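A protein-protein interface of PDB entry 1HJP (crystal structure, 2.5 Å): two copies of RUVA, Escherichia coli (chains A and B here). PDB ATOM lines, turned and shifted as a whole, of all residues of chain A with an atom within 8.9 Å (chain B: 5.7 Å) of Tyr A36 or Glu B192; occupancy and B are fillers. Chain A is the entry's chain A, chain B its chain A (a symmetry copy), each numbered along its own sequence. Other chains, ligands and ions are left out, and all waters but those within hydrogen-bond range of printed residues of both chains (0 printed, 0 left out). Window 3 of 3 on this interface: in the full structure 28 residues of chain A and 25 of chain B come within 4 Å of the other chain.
N of Met A32 sits at hydrogen-bond distance from OG of Ser A91 (2.9 Å).
The backbone NH (N) of Glu B192 lies close to the side-chain hydroxyl (OG) of Ser B190 (3.5 Å).
Ile B195 touches Met A32.
CE1 of Phe A35 touches OE2 of Glu B192, 3.6 Å away.
Tyr A36 touches Glu B192.
Arg B196 touches Tyr A36.
Leu B199 touches Ser A91 (CD2 to O, 3.97 Å).
Of the 9 printed residues of chain B, 4 touch a printed residue of chain A.
Hydrophobic or aromatic side chains of chain B within 4 Å of the printed part of chain A: Ile B195 and Leu B199.
Hydrophobic or aromatic side chains of chain A that line the printed part of chain B: Met A32, Phe A35 and Tyr A36.
Among the printed residues, 5 pairs touch across the chains.
Among the printed residues, no Asp or Glu carboxylate lies within 4 Å of a Lys or Arg side-chain nitrogen of the other chain.
No position is printed for both chains.
Of chain B, only Glu B192 and Arg B196 come within 4 Å of Tyr A36.
Glu B192 touches two residues of chain A.
No residue of chain A comes within 4 Å of Ser B191.
No residue of chain A comes within 4 Å of Thr B193.
Printed residues of chain B within 4 Å of Phe A35: Glu B192.
Of the printed residues of chain B, Ser A91 touches Leu B199 (3.97 Å).
Of the printed residues of chain A, Leu B199 touches Ser A91 (3.97 Å).
Printed residues of chain A within 4 Å of Arg B196: Tyr A36.
Printed residues of chain B within 4 Å of Met A32: Ile B195.
Glu B197 touches none of the printed residues of chain A.
Ala A41 touches none of the printed residues of chain B.
The nearest residue of chain A that does not touch Glu B192 is Lys A12 (4.1 Å).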
ATOM      1  N   GLU A  11       1.891   9.078  26.587  1.00  0.00           N
ATOM      2  CA  GLU A  11       1.511   8.919  25.202  1.00  0.00           C
ATOM      3  C   GLU A  11       2.139   7.653  24.605  1.00  0.00           C
ATOM      4  O   GLU A  11       3.251   7.284  24.943  1.00  0.00           O
ATOM      5  CB  GLU A  11       1.951  10.041  24.275  1.00  0.00           C
ATOM      6  CG  GLU A  11       1.981  11.463  24.742  1.00  0.00           C
ATOM      7  CD  GLU A  11       2.493  12.457  23.719  1.00  0.00           C
ATOM      8  OE1 GLU A  11       3.023  12.036  22.670  1.00  0.00           O
ATOM      9  OE2 GLU A  11       2.350  13.672  23.985  1.00  0.00           O
ATOM     10  N   LYS A  12       1.444   7.076  23.638  1.00  0.00           N
ATOM     11  CA  LYS A  12       1.991   5.941  22.901  1.00  0.00           C
ATOM     12  C   LYS A  12       2.104   6.338  21.435  1.00  0.00           C
ATOM     13  O   LYS A  12       1.119   6.782  20.866  1.00  0.00           O
ATOM     14  CB  LYS A  12       1.116   4.709  23.046  1.00  0.00           C
ATOM     15  CG  LYS A  12       0.947   4.127  24.443  1.00  0.00           C
ATOM     16  CD  LYS A  12       0.078   2.876  24.331  1.00  0.00           C
ATOM     17  CE  LYS A  12      -0.354   2.373  25.685  1.00  0.00           C
ATOM     18  NZ  LYS A  12      -0.696   0.915  25.696  1.00  0.00           N
ATOM     19  N   GLN A  13       3.242   6.215  20.803  1.00  0.00           N
ATOM     20  CA  GLN A  13       3.456   6.488  19.393  1.00  0.00           C
ATOM     21  C   GLN A  13       4.454   5.430  18.896  1.00  0.00           C
ATOM     22  O   GLN A  13       5.636   5.721  18.717  1.00  0.00           O
ATOM     23  CB  GLN A  13       4.070   7.858  19.168  1.00  0.00           C
ATOM     24  CG  GLN A  13       3.077   8.997  19.009  1.00  0.00           C
ATOM     25  CD  GLN A  13       3.779  10.325  19.270  1.00  0.00           C
ATOM     26  OE1 GLN A  13       3.316  11.111  20.098  1.00  0.00           O
ATOM     27  NE2 GLN A  13       4.889  10.538  18.567  1.00  0.00           N
ATOM     28  N   PRO A  14       3.973   4.205  18.741  1.00  0.00           N
ATOM     29  CA  PRO A  14       4.811   3.070  18.403  1.00  0.00           C
ATOM     30  C   PRO A  14       5.808   3.392  17.315  1.00  0.00           C
ATOM     31  O   PRO A  14       5.429   4.002  16.318  1.00  0.00           O
ATOM     32  CB  PRO A  14       3.846   1.963  18.026  1.00  0.00           C
ATOM     33  CG  PRO A  14       2.473   2.477  18.221  1.00  0.00           C
ATOM     34  CD  PRO A  14       2.565   3.797  18.934  1.00  0.00           C
ATOM     35  N   PRO A  15       7.063   3.023  17.537  1.00  0.00           N
ATOM     36  CA  PRO A  15       7.496   2.284  18.694  1.00  0.00           C
ATOM     37  C   PRO A  15       7.887   3.062  19.939  1.00  0.00           C
ATOM     38  O   PRO A  15       8.449   2.503  20.892  1.00  0.00           O
ATOM     39  CB  PRO A  15       8.725   1.532  18.179  1.00  0.00           C
ATOM     40  CG  PRO A  15       9.202   2.227  16.965  1.00  0.00           C
ATOM     41  CD  PRO A  15       8.167   3.236  16.561  1.00  0.00           C
ATOM     42  N   LEU A  16       7.553   4.331  20.043  1.00  0.00           N
ATOM     43  CA  LEU A  16       7.877   5.178  21.164  1.00  0.00           C
ATOM     44  C   LEU A  16       6.837   5.242  22.260  1.00  0.00           C
ATOM     45  O   LEU A  16       5.641   5.347  21.997  1.00  0.00           O
ATOM     46  CB  LEU A  16       8.054   6.596  20.595  1.00  0.00           C
ATOM     47  CG  LEU A  16       9.081   7.487  21.276  1.00  0.00           C
ATOM     48  CD1 LEU A  16      10.488   7.162  20.790  1.00  0.00           C
ATOM     49  CD2 LEU A  16       8.747   8.949  21.038  1.00  0.00           C
ATOM     50  N   VAL A  17       7.240   5.184  23.524  1.00  0.00           N
ATOM     51  CA  VAL A  17       6.322   5.399  24.626  1.00  0.00           C
ATOM     52  C   VAL A  17       6.891   6.619  25.395  1.00  0.00           C
ATOM     53  O   VAL A  17       8.113   6.755  25.518  1.00  0.00           O
ATOM     54  CB  VAL A  17       6.203   4.333  25.727  1.00  0.00           C
ATOM     55  CG1 VAL A  17       4.762   4.172  26.177  1.00  0.00           C
ATOM     56  CG2 VAL A  17       6.879   3.044  25.359  1.00  0.00           C
ATOM     57  N   MET A  30      10.503   0.881  22.246  1.00  0.00           N
ATOM     58  CA  MET A  30      10.207  -0.518  22.548  1.00  0.00           C
ATOM     59  C   MET A  30       9.855  -1.309  21.296  1.00  0.00           C
ATOM     60  O   MET A  30       9.152  -0.803  20.431  1.00  0.00           O
ATOM     61  CB  MET A  30       9.001  -0.666  23.483  1.00  0.00           C
ATOM     62  CG  MET A  30       8.997   0.122  24.767  1.00  0.00           C
ATOM     63  SD  MET A  30       7.674  -0.239  25.918  1.00  0.00           S
ATOM     64  CE  MET A  30       7.903  -1.926  26.443  1.00  0.00           C
ATOM     65  N   PRO A  31      10.297  -2.559  21.225  1.00  0.00           N
ATOM     66  CA  PRO A  31       9.908  -3.459  20.143  1.00  0.00           C
ATOM     67  C   PRO A  31       8.398  -3.618  20.133  1.00  0.00           C
ATOM     68  O   PRO A  31       7.737  -3.625  21.181  1.00  0.00           O
ATOM     69  CB  PRO A  31      10.611  -4.764  20.471  1.00  0.00           C
ATOM     70  CG  PRO A  31      11.252  -4.645  21.802  1.00  0.00           C
ATOM     71  CD  PRO A  31      11.114  -3.229  22.263  1.00  0.00           C
ATOM     72  N   MET A  32       7.770  -3.762  18.970  1.00  0.00           N
ATOM     73  CA  MET A  32       6.309  -3.902  18.898  1.00  0.00           C
ATOM     74  C   MET A  32       5.714  -5.029  19.720  1.00  0.00           C
ATOM     75  O   MET A  32       4.644  -4.847  20.322  1.00  0.00           O
ATOM     76  CB  MET A  32       5.805  -4.035  17.460  1.00  0.00           C
ATOM     77  CG  MET A  32       5.982  -2.753  16.673  1.00  0.00           C
ATOM     78  SD  MET A  32       5.297  -1.284  17.446  1.00  0.00           S
ATOM     79  CE  MET A  32       3.748  -1.825  18.140  1.00  0.00           C
ATOM     80  N   THR A  33       6.388  -6.168  19.844  1.00  0.00           N
ATOM     81  CA  THR A  33       5.817  -7.265  20.632  1.00  0.00           C
ATOM     82  C   THR A  33       5.766  -6.940  22.107  1.00  0.00           C
ATOM     83  O   THR A  33       4.958  -7.556  22.805  1.00  0.00           O
ATOM     84  CB  THR A  33       6.503  -8.607  20.364  1.00  0.00           C
ATOM     85  OG1 THR A  33       7.875  -8.565  20.755  1.00  0.00           O
ATOM     86  CG2 THR A  33       6.426  -8.923  18.876  1.00  0.00           C
ATOM     87  N   CYS A  34       6.556  -6.006  22.627  1.00  0.00           N
ATOM     88  CA  CYS A  34       6.461  -5.584  24.016  1.00  0.00           C
ATOM     89  C   CYS A  34       5.402  -4.490  24.082  1.00  0.00           C
ATOM     90  O   CYS A  34       4.621  -4.435  25.025  1.00  0.00           O
ATOM     91  CB  CYS A  34       7.743  -5.027  24.600  1.00  0.00           C
ATOM     92  SG  CYS A  34       9.164  -6.105  24.436  1.00  0.00           S
ATOM     93  N   PHE A  35       5.372  -3.679  23.028  1.00  0.00           N
ATOM     94  CA  PHE A  35       4.405  -2.600  22.917  1.00  0.00           C
ATOM     95  C   PHE A  35       2.974  -3.061  23.106  1.00  0.00           C
ATOM     96  O   PHE A  35       2.201  -2.386  23.788  1.00  0.00           O
ATOM     97  CB  PHE A  35       4.540  -1.874  21.556  1.00  0.00           C
ATOM     98  CG  PHE A  35       4.235  -0.405  21.698  1.00  0.00           C
ATOM     99  CD1 PHE A  35       2.935   0.039  21.819  1.00  0.00           C
ATOM    100  CD2 PHE A  35       5.254   0.527  21.744  1.00  0.00           C
ATOM    101  CE1 PHE A  35       2.663   1.385  21.983  1.00  0.00           C
ATOM    102  CE2 PHE A  35       4.995   1.873  21.911  1.00  0.00           C
ATOM    103  CZ  PHE A  35       3.696   2.308  22.022  1.00  0.00           C
ATOM    104  N   TYR A  36       2.574  -4.201  22.550  1.00  0.00           N
ATOM    105  CA  TYR A  36       1.197  -4.676  22.689  1.00  0.00           C
ATOM    106  C   TYR A  36       0.796  -4.898  24.131  1.00  0.00           C
ATOM    107  O   TYR A  36      -0.343  -4.664  24.528  1.00  0.00           O
ATOM    108  CB  TYR A  36       0.969  -5.948  21.853  1.00  0.00           C
ATOM    109  CG  TYR A  36       1.414  -5.825  20.405  1.00  0.00           C
ATOM    110  CD1 TYR A  36       1.117  -4.721  19.622  1.00  0.00           C
ATOM    111  CD2 TYR A  36       2.166  -6.836  19.824  1.00  0.00           C
ATOM    112  CE1 TYR A  36       1.536  -4.623  18.305  1.00  0.00           C
ATOM    113  CE2 TYR A  36       2.609  -6.750  18.526  1.00  0.00           C
ATOM    114  CZ  TYR A  36       2.282  -5.646  17.771  1.00  0.00           C
ATOM    115  OH  TYR A  36       2.735  -5.580  16.470  1.00  0.00           O
ATOM    116  N   GLU A  37       1.704  -5.318  24.993  1.00  0.00           N
ATOM    117  CA  GLU A  37       1.457  -5.596  26.390  1.00  0.00           C
ATOM    118  C   GLU A  37       1.407  -4.402  27.320  1.00  0.00           C
ATOM    119  O   GLU A  37       1.053  -4.605  28.491  1.00  0.00           O
ATOM    120  CB  GLU A  37       2.522  -6.602  26.874  1.00  0.00           C
ATOM    121  CG  GLU A  37       2.440  -7.920  26.121  1.00  0.00           C
ATOM    122  CD  GLU A  37       1.026  -8.468  26.019  1.00  0.00           C
ATOM    123  OE1 GLU A  37       0.330  -8.556  27.057  1.00  0.00           O
ATOM    124  OE2 GLU A  37       0.593  -8.800  24.890  1.00  0.00           O
ATOM    125  N   LEU A  38       1.682  -3.185  26.855  1.00  0.00           N
ATOM    126  CA  LEU A  38       1.656  -2.042  27.747  1.00  0.00           C
ATOM    127  C   LEU A  38       0.272  -1.731  28.278  1.00  0.00           C
ATOM    128  O   LEU A  38      -0.709  -1.780  27.558  1.00  0.00           O
ATOM    129  CB  LEU A  38       2.136  -0.759  27.070  1.00  0.00           C
ATOM    130  CG  LEU A  38       3.607  -0.675  26.680  1.00  0.00           C
ATOM    131  CD1 LEU A  38       3.832   0.488  25.723  1.00  0.00           C
ATOM    132  CD2 LEU A  38       4.481  -0.537  27.915  1.00  0.00           C
ATOM    133  N   PRO A  39       0.209  -1.275  29.523  1.00  0.00           N
ATOM    134  CA  PRO A  39      -1.036  -0.797  30.098  1.00  0.00           C
ATOM    135  C   PRO A  39      -1.513   0.368  29.247  1.00  0.00           C
ATOM    136  O   PRO A  39      -0.914   0.784  28.257  1.00  0.00           O
ATOM    137  CB  PRO A  39      -0.647  -0.335  31.490  1.00  0.00           C
ATOM    138  CG  PRO A  39       0.678  -0.920  31.770  1.00  0.00           C
ATOM    139  CD  PRO A  39       1.357  -1.117  30.447  1.00  0.00           C
ATOM    140  N   GLU A  40      -2.592   0.983  29.668  1.00  0.00           N
ATOM    141  CA  GLU A  40      -3.268   2.086  29.017  1.00  0.00           C
ATOM    142  C   GLU A  40      -2.709   3.439  29.443  1.00  0.00           C
ATOM    143  O   GLU A  40      -2.201   3.576  30.561  1.00  0.00           O
ATOM    144  CB  GLU A  40      -4.759   1.943  29.320  1.00  0.00           C
ATOM    145  CG  GLU A  40      -5.215   1.454  30.657  1.00  0.00           C
ATOM    146  CD  GLU A  40      -4.791   0.177  31.325  1.00  0.00           C
ATOM    147  OE1 GLU A  40      -4.360  -0.819  30.701  1.00  0.00           O
ATOM    148  OE2 GLU A  40      -4.861   0.101  32.578  1.00  0.00           O
ATOM    149  N   ALA A  41      -2.765   4.435  28.557  1.00  0.00           N
ATOM    150  CA  ALA A  41      -2.264   5.762  28.886  1.00  0.00           C
ATOM    151  C   ALA A  41      -2.941   6.244  30.154  1.00  0.00           C
ATOM    152  O   ALA A  41      -4.129   6.022  30.341  1.00  0.00           O
ATOM    153  CB  ALA A  41      -2.441   6.723  27.735  1.00  0.00           C
ATOM    154  N   ASN A  64       9.475  -5.467  28.488  1.00  0.00           N
ATOM    155  CA  ASN A  64       8.630  -5.785  29.626  1.00  0.00           C
ATOM    156  C   ASN A  64       9.295  -6.722  30.629  1.00  0.00           C
ATOM    157  O   ASN A  64       8.828  -6.743  31.778  1.00  0.00           O
ATOM    158  CB  ASN A  64       7.278  -6.358  29.230  1.00  0.00           C
ATOM    159  CG  ASN A  64       6.521  -5.433  28.304  1.00  0.00           C
ATOM    160  OD1 ASN A  64       6.330  -5.756  27.130  1.00  0.00           O
ATOM    161  ND2 ASN A  64       6.079  -4.292  28.792  1.00  0.00           N
ATOM    162  N   LEU A  90      12.709  -7.845  17.029  1.00  0.00           N
ATOM    163  CA  LEU A  90      11.737  -8.113  18.086  1.00  0.00           C
ATOM    164  C   LEU A  90      10.384  -7.467  17.852  1.00  0.00           C
ATOM    165  O   LEU A  90       9.477  -7.510  18.701  1.00  0.00           O
ATOM    166  CB  LEU A  90      12.371  -7.711  19.407  1.00  0.00           C
ATOM    167  CG  LEU A  90      13.114  -8.714  20.269  1.00  0.00           C
ATOM    168  CD1 LEU A  90      13.510  -9.976  19.529  1.00  0.00           C
ATOM    169  CD2 LEU A  90      14.375  -8.086  20.863  1.00  0.00           C
ATOM    170  N   SER A  91      10.160  -6.846  16.703  1.00  0.00           N
ATOM    171  CA  SER A  91       8.878  -6.254  16.349  1.00  0.00           C
ATOM    172  C   SER A  91       8.136  -7.249  15.459  1.00  0.00           C
ATOM    173  O   SER A  91       6.952  -7.511  15.593  1.00  0.00           O
ATOM    174  CB  SER A  91       9.037  -4.947  15.583  1.00  0.00           C
ATOM    175  OG  SER A  91       9.258  -3.883  16.495  1.00  0.00           O
ATOM    176  N   GLY A  92       8.938  -7.843  14.570  1.00  0.00           N
ATOM    177  CA  GLY A  92       8.457  -8.831  13.622  1.00  0.00           C
ATOM    178  C   GLY A  92       8.142 -10.142  14.327  1.00  0.00           C
ATOM    179  O   GLY A  92       7.238 -10.866  13.883  1.00  0.00           O
ATOM    180  N   MET A  93       8.861 -10.466  15.391  1.00  0.00           N
ATOM    181  CA  MET A  93       8.564 -11.709  16.097  1.00  0.00           C
ATOM    182  C   MET A  93       8.842 -11.573  17.586  1.00  0.00           C
ATOM    183  O   MET A  93       9.598 -10.704  18.026  1.00  0.00           O
ATOM    184  CB  MET A  93       9.269 -12.898  15.472  1.00  0.00           C
ATOM    185  CG  MET A  93      10.769 -12.955  15.395  1.00  0.00           C
ATOM    186  SD  MET A  93      11.370 -14.119  14.140  1.00  0.00           S
ATOM    187  CE  MET A  93      12.788 -13.204  13.536  1.00  0.00           C
ATOM    188  N   SER A  94       8.167 -12.419  18.364  1.00  0.00           N
ATOM    189  CA  SER A  94       8.359 -12.394  19.809  1.00  0.00           C
ATOM    190  C   SER A  94       9.742 -12.962  20.121  1.00  0.00           C
ATOM    191  O   SER A  94      10.398 -13.560  19.265  1.00  0.00           O
ATOM    192  CB  SER A  94       7.291 -13.191  20.541  1.00  0.00           C
ATOM    193  OG  SER A  94       7.619 -14.576  20.521  1.00  0.00           O
ATOM    194  N   SER B 190      -7.469   0.353  15.467  1.00  0.00           N
ATOM    195  CA  SER B 190      -6.248   0.820  16.093  1.00  0.00           C
ATOM    196  C   SER B 190      -5.000   0.738  15.223  1.00  0.00           C
ATOM    197  O   SER B 190      -4.817  -0.188  14.430  1.00  0.00           O
ATOM    198  CB  SER B 190      -5.991  -0.011  17.363  1.00  0.00           C
ATOM    199  OG  SER B 190      -5.188  -1.138  17.063  1.00  0.00           O
ATOM    200  N   SER B 191      -4.070   1.661  15.457  1.00  0.00           N
ATOM    201  CA  SER B 191      -2.804   1.704  14.741  1.00  0.00           C
ATOM    202  C   SER B 191      -1.909   0.514  15.070  1.00  0.00           C
ATOM    203  O   SER B 191      -1.126   0.053  14.239  1.00  0.00           O
ATOM    204  CB  SER B 191      -2.072   3.008  15.056  1.00  0.00           C
ATOM    205  OG  SER B 191      -1.659   3.064  16.406  1.00  0.00           O
ATOM    206  N   GLU B 192      -2.021   0.006  16.293  1.00  0.00           N
ATOM    207  CA  GLU B 192      -1.266  -1.134  16.761  1.00  0.00           C
ATOM    208  C   GLU B 192      -1.665  -2.429  16.077  1.00  0.00           C
ATOM    209  O   GLU B 192      -0.791  -3.178  15.642  1.00  0.00           O
ATOM    210  CB  GLU B 192      -1.435  -1.296  18.274  1.00  0.00           C
ATOM    211  CG  GLU B 192      -0.268  -0.689  19.047  1.00  0.00           C
ATOM    212  CD  GLU B 192      -0.686  -0.440  20.484  1.00  0.00           C
ATOM    213  OE1 GLU B 192      -1.014  -1.449  21.130  1.00  0.00           O
ATOM    214  OE2 GLU B 192      -0.694   0.729  20.907  1.00  0.00           O
ATOM    215  N   THR B 193      -2.968  -2.678  15.947  1.00  0.00           N
ATOM    216  CA  THR B 193      -3.438  -3.880  15.248  1.00  0.00           C
ATOM    217  C   THR B 193      -3.060  -3.777  13.770  1.00  0.00           C
ATOM    218  O   THR B 193      -2.614  -4.758  13.175  1.00  0.00           O
ATOM    219  CB  THR B 193      -4.947  -4.115  15.386  1.00  0.00           C
ATOM    220  OG1 THR B 193      -5.622  -3.037  14.718  1.00  0.00           O
ATOM    221  CG2 THR B 193      -5.355  -4.157  16.851  1.00  0.00           C
ATOM    222  N   LEU B 194      -3.133  -2.575  13.206  1.00  0.00           N
ATOM    223  CA  LEU B 194      -2.664  -2.335  11.853  1.00  0.00           C
ATOM    224  C   LEU B 194      -1.189  -2.706  11.731  1.00  0.00           C
ATOM    225  O   LEU B 194      -0.804  -3.352  10.758  1.00  0.00           O
ATOM    226  CB  LEU B 194      -2.850  -0.869  11.457  1.00  0.00           C
ATOM    227  CG  LEU B 194      -4.173  -0.505  10.778  1.00  0.00           C
ATOM    228  CD1 LEU B 194      -4.740   0.784  11.346  1.00  0.00           C
ATOM    229  CD2 LEU B 194      -3.966  -0.398   9.274  1.00  0.00           C
ATOM    230  N   ILE B 195      -0.362  -2.314  12.702  1.00  0.00           N
ATOM    231  CA  ILE B 195       1.057  -2.657  12.697  1.00  0.00           C
ATOM    232  C   ILE B 195       1.224  -4.165  12.886  1.00  0.00           C
ATOM    233  O   ILE B 195       2.032  -4.795  12.209  1.00  0.00           O
ATOM    234  CB  ILE B 195       1.856  -1.891  13.763  1.00  0.00           C
ATOM    235  CG1 ILE B 195       1.835  -0.381  13.495  1.00  0.00           C
ATOM    236  CG2 ILE B 195       3.310  -2.347  13.850  1.00  0.00           C
ATOM    237  CD1 ILE B 195       1.925   0.456  14.751  1.00  0.00           C
ATOM    238  N   ARG B 196       0.451  -4.760  13.787  1.00  0.00           N
ATOM    239  CA  ARG B 196       0.518  -6.193  14.015  1.00  0.00           C
ATOM    240  C   ARG B 196       0.098  -6.958  12.764  1.00  0.00           C
ATOM    241  O   ARG B 196       0.815  -7.849  12.304  1.00  0.00           O
ATOM    242  CB  ARG B 196      -0.339  -6.623  15.203  1.00  0.00           C
ATOM    243  CG  ARG B 196       0.068  -7.988  15.735  1.00  0.00           C
ATOM    244  CD  ARG B 196      -0.850  -8.491  16.835  1.00  0.00           C
ATOM    245  NE  ARG B 196      -1.059  -7.496  17.877  1.00  0.00           N
ATOM    246  CZ  ARG B 196      -2.179  -6.793  18.030  1.00  0.00           C
ATOM    247  NH1 ARG B 196      -3.200  -6.986  17.201  1.00  0.00           N
ATOM    248  NH2 ARG B 196      -2.267  -5.901  19.012  1.00  0.00           N
ATOM    249  N   GLU B 197      -1.047  -6.576  12.194  1.00  0.00           N
ATOM    250  CA  GLU B 197      -1.558  -7.218  10.994  1.00  0.00           C
ATOM    251  C   GLU B 197      -0.629  -7.015   9.804  1.00  0.00           C
ATOM    252  O   GLU B 197      -0.359  -7.980   9.085  1.00  0.00           O
ATOM    253  CB  GLU B 197      -2.962  -6.742  10.634  1.00  0.00           C
ATOM    254  CG  GLU B 197      -4.043  -6.971  11.662  1.00  0.00           C
ATOM    255  CD  GLU B 197      -4.420  -8.407  11.946  1.00  0.00           C
ATOM    256  OE1 GLU B 197      -3.523  -9.251  12.168  1.00  0.00           O
ATOM    257  OE2 GLU B 197      -5.640  -8.702  11.966  1.00  0.00           O
ATOM    258  N   LEU B 199       2.624  -6.437   9.771  1.00  0.00           N
ATOM    259  CA  LEU B 199       3.907  -7.096   9.990  1.00  0.00           C
ATOM    260  C   LEU B 199       3.753  -8.606   9.849  1.00  0.00           C
ATOM    261  O   LEU B 199       4.661  -9.288   9.376  1.00  0.00           O
ATOM    262  CB  LEU B 199       4.448  -6.702  11.354  1.00  0.00           C
ATOM    263  CG  LEU B 199       5.876  -6.215  11.539  1.00  0.00           C
ATOM    264  CD1 LEU B 199       6.531  -5.728  10.259  1.00  0.00           C
ATOM    265  CD2 LEU B 199       5.905  -5.119  12.598  1.00  0.00           C
